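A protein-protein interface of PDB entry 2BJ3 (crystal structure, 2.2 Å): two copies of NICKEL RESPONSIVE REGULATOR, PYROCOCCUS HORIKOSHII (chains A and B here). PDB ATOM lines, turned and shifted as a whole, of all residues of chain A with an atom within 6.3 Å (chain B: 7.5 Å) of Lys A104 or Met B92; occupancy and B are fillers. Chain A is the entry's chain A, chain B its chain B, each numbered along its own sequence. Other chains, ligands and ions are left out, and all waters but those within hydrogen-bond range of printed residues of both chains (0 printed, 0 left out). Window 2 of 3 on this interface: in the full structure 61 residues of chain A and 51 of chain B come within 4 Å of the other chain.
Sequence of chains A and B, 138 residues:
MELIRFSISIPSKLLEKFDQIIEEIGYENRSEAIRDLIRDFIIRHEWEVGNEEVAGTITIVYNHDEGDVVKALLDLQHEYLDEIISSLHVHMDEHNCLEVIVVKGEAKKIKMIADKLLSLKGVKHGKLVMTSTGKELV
The side-chain amino group (NZ) of Lys A104 lies within hydrogen-bond range of the backbone carbonyl oxygen (O) of Met B92 (3.2 Å).
Printed residues of chain B that touch a printed residue of chain A: Met B92, Asp B93, Asn B96 and Leu B98. Hydrophobic or aromatic side chains of chain B that line the printed part of chain A: Met B92 and Leu B98. Of the 15 printed residues of chain A, 7 touch a printed residue of chain B. Hydrophobic or aromatic side chains of chain A within 4 Å of the printed part of chain B: Ala A55, Ile A85 and Val A102. Among the printed residues, no Asp or Glu carboxylate lies within 4 Å of a Lys or Arg side-chain nitrogen of the other chain.
The backbone carbonyl oxygen (O) of Gly A56 is in hydrogen-bond range of the backbone NH (N) of Val A103 (3.0 Å). The backbone carbonyl oxygen (O) of Val B90 sits at hydrogen-bond distance from the backbone NH (N) of Leu B98, 2.9 Å away. The side-chain hydroxyl (OG1) of Thr A133 sits at hydrogen-bond distance from the side-chain carboxylate (OE1) of Glu A53 (2.5 Å). OD1 of Asp B93 sits close to N of His B95 (3.3 Å). The backbone NH of Lys A104 sits at hydrogen-bond distance from the backbone carbonyl oxygen of Glu A83, at 2.9 Å. The side-chain carboxylate of Glu A53 lies within salt-bridge range of the side-chain amino group of Lys A104 (3.9 Å).
Ala A55 touches Met B92. Leu B98 touches Gly A56 (CD1 to O, 3.7 Å). Ile A85 touches Met B92 (CD1 to CE, 3.1 Å). CG1 of Val A102 touches CD1 of Leu B98, 3.7 Å away. O of Val A103 touches CE of Met B92, at 3.7 Å. Thr A133 touches Asp B93. Thr A133 touches Asn B96.
Of chain B, only Met B92 (3.2 Å) comes within 4 Å of Lys A104. Of the printed residues of chain A, Met B92 touches Ala A55, Ile A85, Val A103 and Lys A104. Of the printed residues of chain B, Gly A56 touches Leu B98 (3.7 Å). Printed residues of chain B within 4 Å of Val A103: Met B92. Of the printed residues of chain B, Ala A55 touches Met B92 (3.3 Å). His B95 touches none of the printed residues of chain A. Val A54 touches none of the printed residues of chain B. The nearest residue of chain A that does not touch Met B92 is Val A102 (4.7 Å).
No position is printed for both chains.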
ATOM      1  N   GLU A  53      15.239 -21.791 -11.476  1.00  0.00           N
ATOM      2  CA  GLU A  53      16.680 -21.671 -11.329  1.00  0.00           C
ATOM      3  C   GLU A  53      17.231 -22.896 -10.621  1.00  0.00           C
ATOM      4  O   GLU A  53      16.661 -23.369  -9.640  1.00  0.00           O
ATOM      5  CB  GLU A  53      17.050 -20.415 -10.537  1.00  0.00           C
ATOM      6  CG  GLU A  53      18.553 -20.267 -10.287  1.00  0.00           C
ATOM      7  CD  GLU A  53      18.911 -19.050  -9.438  1.00  0.00           C
ATOM      8  OE1 GLU A  53      18.391 -18.933  -8.307  1.00  0.00           O
ATOM      9  OE2 GLU A  53      19.717 -18.212  -9.899  1.00  0.00           O
ATOM     10  N   VAL A  54      18.339 -23.412 -11.136  1.00  0.00           N
ATOM     11  CA  VAL A  54      18.981 -24.573 -10.556  1.00  0.00           C
ATOM     12  C   VAL A  54      20.472 -24.341 -10.461  1.00  0.00           C
ATOM     13  O   VAL A  54      21.030 -23.472 -11.126  1.00  0.00           O
ATOM     14  CB  VAL A  54      18.739 -25.838 -11.390  1.00  0.00           C
ATOM     15  CG1 VAL A  54      17.300 -26.237 -11.306  1.00  0.00           C
ATOM     16  CG2 VAL A  54      19.140 -25.597 -12.835  1.00  0.00           C
ATOM     17  N   ALA A  55      21.116 -25.127  -9.611  1.00  0.00           N
ATOM     18  CA  ALA A  55      22.551 -25.022  -9.418  1.00  0.00           C
ATOM     19  C   ALA A  55      23.017 -26.455  -9.182  1.00  0.00           C
ATOM     20  O   ALA A  55      22.230 -27.303  -8.776  1.00  0.00           O
ATOM     21  CB  ALA A  55      22.846 -24.143  -8.214  1.00  0.00           C
ATOM     22  N   GLY A  56      24.284 -26.737  -9.439  1.00  0.00           N
ATOM     23  CA  GLY A  56      24.744 -28.097  -9.258  1.00  0.00           C
ATOM     24  C   GLY A  56      25.959 -28.366 -10.107  1.00  0.00           C
ATOM     25  O   GLY A  56      26.728 -27.451 -10.393  1.00  0.00           O
ATOM     26  N   ASP A  82      28.210 -17.208 -17.976  1.00  0.00           N
ATOM     27  CA  ASP A  82      27.293 -16.598 -17.018  1.00  0.00           C
ATOM     28  C   ASP A  82      26.710 -17.684 -16.127  1.00  0.00           C
ATOM     29  O   ASP A  82      26.380 -17.447 -14.967  1.00  0.00           O
ATOM     30  CB  ASP A  82      26.171 -15.844 -17.741  1.00  0.00           C
ATOM     31  CG  ASP A  82      26.593 -14.449 -18.185  1.00  0.00           C
ATOM     32  OD1 ASP A  82      25.862 -13.836 -18.994  1.00  0.00           O
ATOM     33  OD2 ASP A  82      27.648 -13.962 -17.720  1.00  0.00           O
ATOM     34  N   GLU A  83      26.583 -18.886 -16.671  1.00  0.00           N
ATOM     35  CA  GLU A  83      26.060 -19.983 -15.879  1.00  0.00           C
ATOM     36  C   GLU A  83      27.151 -20.895 -15.295  1.00  0.00           C
ATOM     37  O   GLU A  83      26.902 -21.599 -14.324  1.00  0.00           O
ATOM     38  CB  GLU A  83      25.072 -20.809 -16.702  1.00  0.00           C
ATOM     39  CG  GLU A  83      25.092 -20.512 -18.184  1.00  0.00           C
ATOM     40  CD  GLU A  83      24.355 -19.234 -18.529  1.00  0.00           C
ATOM     41  OE1 GLU A  83      23.146 -19.144 -18.207  1.00  0.00           O
ATOM     42  OE2 GLU A  83      24.989 -18.329 -19.118  1.00  0.00           O
ATOM     43  N   ILE A  84      28.342 -20.868 -15.890  1.00  0.00           N
ATOM     44  CA  ILE A  84      29.484 -21.691 -15.462  1.00  0.00           C
ATOM     45  C   ILE A  84      30.306 -20.964 -14.410  1.00  0.00           C
ATOM     46  O   ILE A  84      31.097 -20.080 -14.743  1.00  0.00           O
ATOM     47  CB  ILE A  84      30.470 -21.966 -16.621  1.00  0.00           C
ATOM     48  CG1 ILE A  84      29.737 -22.515 -17.842  1.00  0.00           C
ATOM     49  CG2 ILE A  84      31.562 -22.925 -16.144  1.00  0.00           C
ATOM     50  CD1 ILE A  84      29.116 -23.818 -17.637  1.00  0.00           C
ATOM     51  N   ILE A  85      30.144 -21.338 -13.149  1.00  0.00           N
ATOM     52  CA  ILE A  85      30.882 -20.671 -12.085  1.00  0.00           C
ATOM     53  C   ILE A  85      32.358 -21.078 -12.012  1.00  0.00           C
ATOM     54  O   ILE A  85      33.222 -20.208 -11.947  1.00  0.00           O
ATOM     55  CB  ILE A  85      30.227 -20.937 -10.733  1.00  0.00           C
ATOM     56  CG1 ILE A  85      28.770 -20.490 -10.787  1.00  0.00           C
ATOM     57  CG2 ILE A  85      30.969 -20.191  -9.634  1.00  0.00           C
ATOM     58  CD1 ILE A  85      28.020 -20.759  -9.513  1.00  0.00           C
ATOM     59  N   VAL A 102      30.772 -26.541 -12.295  1.00  0.00           N
ATOM     60  CA  VAL A 102      29.811 -25.963 -11.356  1.00  0.00           C
ATOM     61  C   VAL A 102      28.963 -24.954 -12.109  1.00  0.00           C
ATOM     62  O   VAL A 102      29.488 -24.024 -12.723  1.00  0.00           O
ATOM     63  CB  VAL A 102      30.506 -25.236 -10.189  1.00  0.00           C
ATOM     64  CG1 VAL A 102      29.459 -24.537  -9.314  1.00  0.00           C
ATOM     65  CG2 VAL A 102      31.290 -26.239  -9.358  1.00  0.00           C
ATOM     66  N   VAL A 103      27.651 -25.131 -12.055  1.00  0.00           N
ATOM     67  CA  VAL A 103      26.765 -24.223 -12.770  1.00  0.00           C
ATOM     68  C   VAL A 103      25.586 -23.709 -11.957  1.00  0.00           C
ATOM     69  O   VAL A 103      25.218 -24.281 -10.929  1.00  0.00           O
ATOM     70  CB  VAL A 103      26.186 -24.908 -14.013  1.00  0.00           C
ATOM     71  CG1 VAL A 103      27.300 -25.413 -14.911  1.00  0.00           C
ATOM     72  CG2 VAL A 103      25.305 -26.034 -13.588  1.00  0.00           C
ATOM     73  N   LYS A 104      24.990 -22.631 -12.457  1.00  0.00           N
ATOM     74  CA  LYS A 104      23.813 -22.021 -11.848  1.00  0.00           C
ATOM     75  C   LYS A 104      23.027 -21.305 -12.950  1.00  0.00           C
ATOM     76  O   LYS A 104      23.599 -20.560 -13.737  1.00  0.00           O
ATOM     77  CB  LYS A 104      24.217 -21.008 -10.779  1.00  0.00           C
ATOM     78  CG  LYS A 104      23.061 -20.491  -9.950  1.00  0.00           C
ATOM     79  CD  LYS A 104      23.496 -19.308  -9.105  1.00  0.00           C
ATOM     80  CE  LYS A 104      22.323 -18.714  -8.351  1.00  0.00           C
ATOM     81  NZ  LYS A 104      22.742 -17.513  -7.586  1.00  0.00           N
ATOM     82  N   GLY A 105      21.721 -21.533 -13.014  1.00  0.00           N
ATOM     83  CA  GLY A 105      20.930 -20.872 -14.036  1.00  0.00           C
ATOM     84  C   GLY A 105      19.572 -21.495 -14.249  1.00  0.00           C
ATOM     85  O   GLY A 105      19.203 -22.448 -13.567  1.00  0.00           O
ATOM     86  N   GLU A 106      18.822 -20.947 -15.197  1.00  0.00           N
ATOM     87  CA  GLU A 106      17.493 -21.453 -15.517  1.00  0.00           C
ATOM     88  C   GLU A 106      17.671 -22.877 -16.025  1.00  0.00           C
ATOM     89  O   GLU A 106      18.519 -23.131 -16.882  1.00  0.00           O
ATOM     90  CB  GLU A 106      16.847 -20.596 -16.613  1.00  0.00           C
ATOM     91  CG  GLU A 106      17.099 -19.101 -16.479  1.00  0.00           C
ATOM     92  CD  GLU A 106      16.403 -18.484 -15.279  1.00  0.00           C
ATOM     93  OE1 GLU A 106      15.154 -18.516 -15.240  1.00  0.00           O
ATOM     94  OE2 GLU A 106      17.104 -17.967 -14.379  1.00  0.00           O
ATOM     95  N   ILE A 110      20.508 -24.612 -18.632  1.00  0.00           N
ATOM     96  CA  ILE A 110      21.455 -25.621 -18.186  1.00  0.00           C
ATOM     97  C   ILE A 110      21.334 -26.891 -19.031  1.00  0.00           C
ATOM     98  O   ILE A 110      22.353 -27.471 -19.430  1.00  0.00           O
ATOM     99  CB  ILE A 110      21.257 -25.961 -16.701  1.00  0.00           C
ATOM    100  CG1 ILE A 110      21.386 -24.690 -15.844  1.00  0.00           C
ATOM    101  CG2 ILE A 110      22.266 -27.016 -16.281  1.00  0.00           C
ATOM    102  CD1 ILE A 110      22.669 -23.912 -16.050  1.00  0.00           C
ATOM    103  N   THR A 133      17.250 -23.841  -6.744  1.00  0.00           N
ATOM    104  CA  THR A 133      17.699 -23.025  -5.617  1.00  0.00           C
ATOM    105  C   THR A 133      16.488 -22.413  -4.890  1.00  0.00           C
ATOM    106  O   THR A 133      15.477 -22.078  -5.508  1.00  0.00           O
ATOM    107  CB  THR A 133      18.668 -21.895  -6.077  1.00  0.00           C
ATOM    108  OG1 THR A 133      18.046 -21.103  -7.091  1.00  0.00           O
ATOM    109  CG2 THR A 133      19.964 -22.486  -6.622  1.00  0.00           C
ATOM    110  N   VAL B  61      24.460 -29.809  -2.295  1.00  0.00           N
ATOM    111  CA  VAL B  61      23.940 -28.454  -2.258  1.00  0.00           C
ATOM    112  C   VAL B  61      23.325 -28.346  -0.877  1.00  0.00           C
ATOM    113  O   VAL B  61      22.552 -29.210  -0.475  1.00  0.00           O
ATOM    114  CB  VAL B  61      22.874 -28.214  -3.359  1.00  0.00           C
ATOM    115  CG1 VAL B  61      22.141 -26.902  -3.093  1.00  0.00           C
ATOM    116  CG2 VAL B  61      23.562 -28.152  -4.729  1.00  0.00           C
ATOM    117  N   HIS B  89      34.378 -25.014  -2.586  1.00  0.00           N
ATOM    118  CA  HIS B  89      33.211 -24.450  -1.922  1.00  0.00           C
ATOM    119  C   HIS B  89      32.724 -23.257  -2.730  1.00  0.00           C
ATOM    120  O   HIS B  89      33.517 -22.490  -3.259  1.00  0.00           O
ATOM    121  CB  HIS B  89      33.543 -24.003  -0.499  1.00  0.00           C
ATOM    122  CG  HIS B  89      32.361 -23.467   0.247  1.00  0.00           C
ATOM    123  ND1 HIS B  89      31.353 -24.277   0.724  1.00  0.00           N
ATOM    124  CD2 HIS B  89      31.990 -22.197   0.536  1.00  0.00           C
ATOM    125  CE1 HIS B  89      30.411 -23.527   1.270  1.00  0.00           C
ATOM    126  NE2 HIS B  89      30.773 -22.261   1.169  1.00  0.00           N
ATOM    127  N   VAL B  90      31.412 -23.127  -2.866  1.00  0.00           N
ATOM    128  CA  VAL B  90      30.839 -21.999  -3.598  1.00  0.00           C
ATOM    129  C   VAL B  90      29.566 -21.507  -2.910  1.00  0.00           C
ATOM    130  O   VAL B  90      28.627 -22.276  -2.676  1.00  0.00           O
ATOM    131  CB  VAL B  90      30.499 -22.357  -5.075  1.00  0.00           C
ATOM    132  CG1 VAL B  90      31.765 -22.568  -5.873  1.00  0.00           C
ATOM    133  CG2 VAL B  90      29.669 -23.615  -5.131  1.00  0.00           C
ATOM    134  N   HIS B  91      29.569 -20.234  -2.542  1.00  0.00           N
ATOM    135  CA  HIS B  91      28.405 -19.622  -1.911  1.00  0.00           C
ATOM    136  C   HIS B  91      27.637 -19.106  -3.119  1.00  0.00           C
ATOM    137  O   HIS B  91      28.090 -18.191  -3.807  1.00  0.00           O
ATOM    138  CB  HIS B  91      28.826 -18.446  -1.037  1.00  0.00           C
ATOM    139  CG  HIS B  91      28.162 -18.414   0.304  1.00  0.00           C
ATOM    140  ND1 HIS B  91      28.628 -19.139   1.380  1.00  0.00           N
ATOM    141  CD2 HIS B  91      27.065 -17.750   0.740  1.00  0.00           C
ATOM    142  CE1 HIS B  91      27.844 -18.921   2.424  1.00  0.00           C
ATOM    143  NE2 HIS B  91      26.889 -18.083   2.061  1.00  0.00           N
ATOM    144  N   MET B  92      26.487 -19.695  -3.397  1.00  0.00           N
ATOM    145  CA  MET B  92      25.724 -19.280  -4.555  1.00  0.00           C
ATOM    146  C   MET B  92      24.762 -18.137  -4.289  1.00  0.00           C
ATOM    147  O   MET B  92      24.705 -17.186  -5.062  1.00  0.00           O
ATOM    148  CB  MET B  92      25.000 -20.488  -5.120  1.00  0.00           C
ATOM    149  CG  MET B  92      25.965 -21.626  -5.369  1.00  0.00           C
ATOM    150  SD  MET B  92      25.311 -22.868  -6.430  1.00  0.00           S
ATOM    151  CE  MET B  92      25.660 -22.140  -7.980  1.00  0.00           C
ATOM    152  N   ASP B  93      24.014 -18.223  -3.198  1.00  0.00           N
ATOM    153  CA  ASP B  93      23.081 -17.164  -2.852  1.00  0.00           C
ATOM    154  C   ASP B  93      22.856 -17.118  -1.345  1.00  0.00           C
ATOM    155  O   ASP B  93      23.421 -17.923  -0.608  1.00  0.00           O
ATOM    156  CB  ASP B  93      21.755 -17.352  -3.602  1.00  0.00           C
ATOM    157  CG  ASP B  93      21.167 -18.743  -3.430  1.00  0.00           C
ATOM    158  OD1 ASP B  93      20.937 -19.164  -2.278  1.00  0.00           O
ATOM    159  OD2 ASP B  93      20.922 -19.413  -4.457  1.00  0.00           O
ATOM    160  N   GLU B  94      22.045 -16.170  -0.893  1.00  0.00           N
ATOM    161  CA  GLU B  94      21.757 -16.011   0.530  1.00  0.00           C
ATOM    162  C   GLU B  94      21.831 -17.313   1.328  1.00  0.00           C
ATOM    163  O   GLU B  94      22.588 -17.410   2.295  1.00  0.00           O
ATOM    164  CB  GLU B  94      20.373 -15.380   0.721  1.00  0.00           C
ATOM    165  CG  GLU B  94      19.959 -15.218   2.184  1.00  0.00           C
ATOM    166  CD  GLU B  94      20.830 -14.226   2.939  1.00  0.00           C
ATOM    167  OE1 GLU B  94      20.728 -14.176   4.185  1.00  0.00           O
ATOM    168  OE2 GLU B  94      21.608 -13.493   2.287  1.00  0.00           O
ATOM    169  N   HIS B  95      21.054 -18.311   0.918  1.00  0.00           N
ATOM    170  CA  HIS B  95      21.020 -19.598   1.611  1.00  0.00           C
ATOM    171  C   HIS B  95      21.969 -20.651   1.054  1.00  0.00           C
ATOM    172  O   HIS B  95      22.929 -21.057   1.708  1.00  0.00           O
ATOM    173  CB  HIS B  95      19.603 -20.181   1.580  1.00  0.00           C
ATOM    174  CG  HIS B  95      18.646 -19.507   2.514  1.00  0.00           C
ATOM    175  ND1 HIS B  95      18.877 -19.403   3.869  1.00  0.00           N
ATOM    176  CD2 HIS B  95      17.445 -18.924   2.291  1.00  0.00           C
ATOM    177  CE1 HIS B  95      17.859 -18.784   4.441  1.00  0.00           C
ATOM    178  NE2 HIS B  95      16.976 -18.483   3.505  1.00  0.00           N
ATOM    179  N   ASN B  96      21.661 -21.082  -0.163  1.00  0.00           N
ATOM    180  CA  ASN B  96      22.383 -22.116  -0.896  1.00  0.00           C
ATOM    181  C   ASN B  96      23.897 -22.110  -1.010  1.00  0.00           C
ATOM    182  O   ASN B  96      24.523 -21.137  -1.432  1.00  0.00           O
ATOM    183  CB  ASN B  96      21.794 -22.217  -2.294  1.00  0.00           C
ATOM    184  CG  ASN B  96      20.311 -22.464  -2.263  1.00  0.00           C
ATOM    185  OD1 ASN B  96      19.853 -23.492  -1.757  1.00  0.00           O
ATOM    186  ND2 ASN B  96      19.542 -21.513  -2.786  1.00  0.00           N
ATOM    187  N   CYS B  97      24.471 -23.245  -0.639  1.00  0.00           N
ATOM    188  CA  CYS B  97      25.906 -23.457  -0.714  1.00  0.00           C
ATOM    189  C   CYS B  97      26.124 -24.727  -1.492  1.00  0.00           C
ATOM    190  O   CYS B  97      25.339 -25.672  -1.397  1.00  0.00           O
ATOM    191  CB  CYS B  97      26.520 -23.618   0.676  1.00  0.00           C
ATOM    192  SG  CYS B  97      26.846 -22.060   1.459  1.00  0.00           S
ATOM    193  N   LEU B  98      27.186 -24.748  -2.275  1.00  0.00           N
ATOM    194  CA  LEU B  98      27.473 -25.940  -3.035  1.00  0.00           C
ATOM    195  C   LEU B  98      28.881 -26.376  -2.672  1.00  0.00           C
ATOM    196  O   LEU B  98      29.790 -25.565  -2.595  1.00  0.00           O
ATOM    197  CB  LEU B  98      27.363 -25.661  -4.536  1.00  0.00           C
ATOM    198  CG  LEU B  98      27.528 -26.853  -5.495  1.00  0.00           C
ATOM    199  CD1 LEU B  98      27.318 -26.397  -6.924  1.00  0.00           C
ATOM    200  CD2 LEU B  98      28.910 -27.441  -5.368  1.00  0.00           C
ATOM    201  N   GLU B  99      29.046 -27.670  -2.460  1.00  0.00           N
ATOM    202  CA  GLU B  99      30.340 -28.245  -2.116  1.00  0.00           C
ATOM    203  C   GLU B  99      30.605 -29.384  -3.110  1.00  0.00           C
ATOM    204  O   GLU B  99      29.727 -30.219  -3.337  1.00  0.00           O
ATOM    205  CB  GLU B  99      30.255 -28.796  -0.690  1.00  0.00           C
ATOM    206  CG  GLU B  99      31.538 -29.304  -0.088  1.00  0.00           C
ATOM    207  CD  GLU B  99      32.531 -28.198   0.169  1.00  0.00           C
ATOM    208  OE1 GLU B  99      32.104 -27.096   0.590  1.00  0.00           O
ATOM    209  OE2 GLU B  99      33.739 -28.435  -0.041  1.00  0.00           O
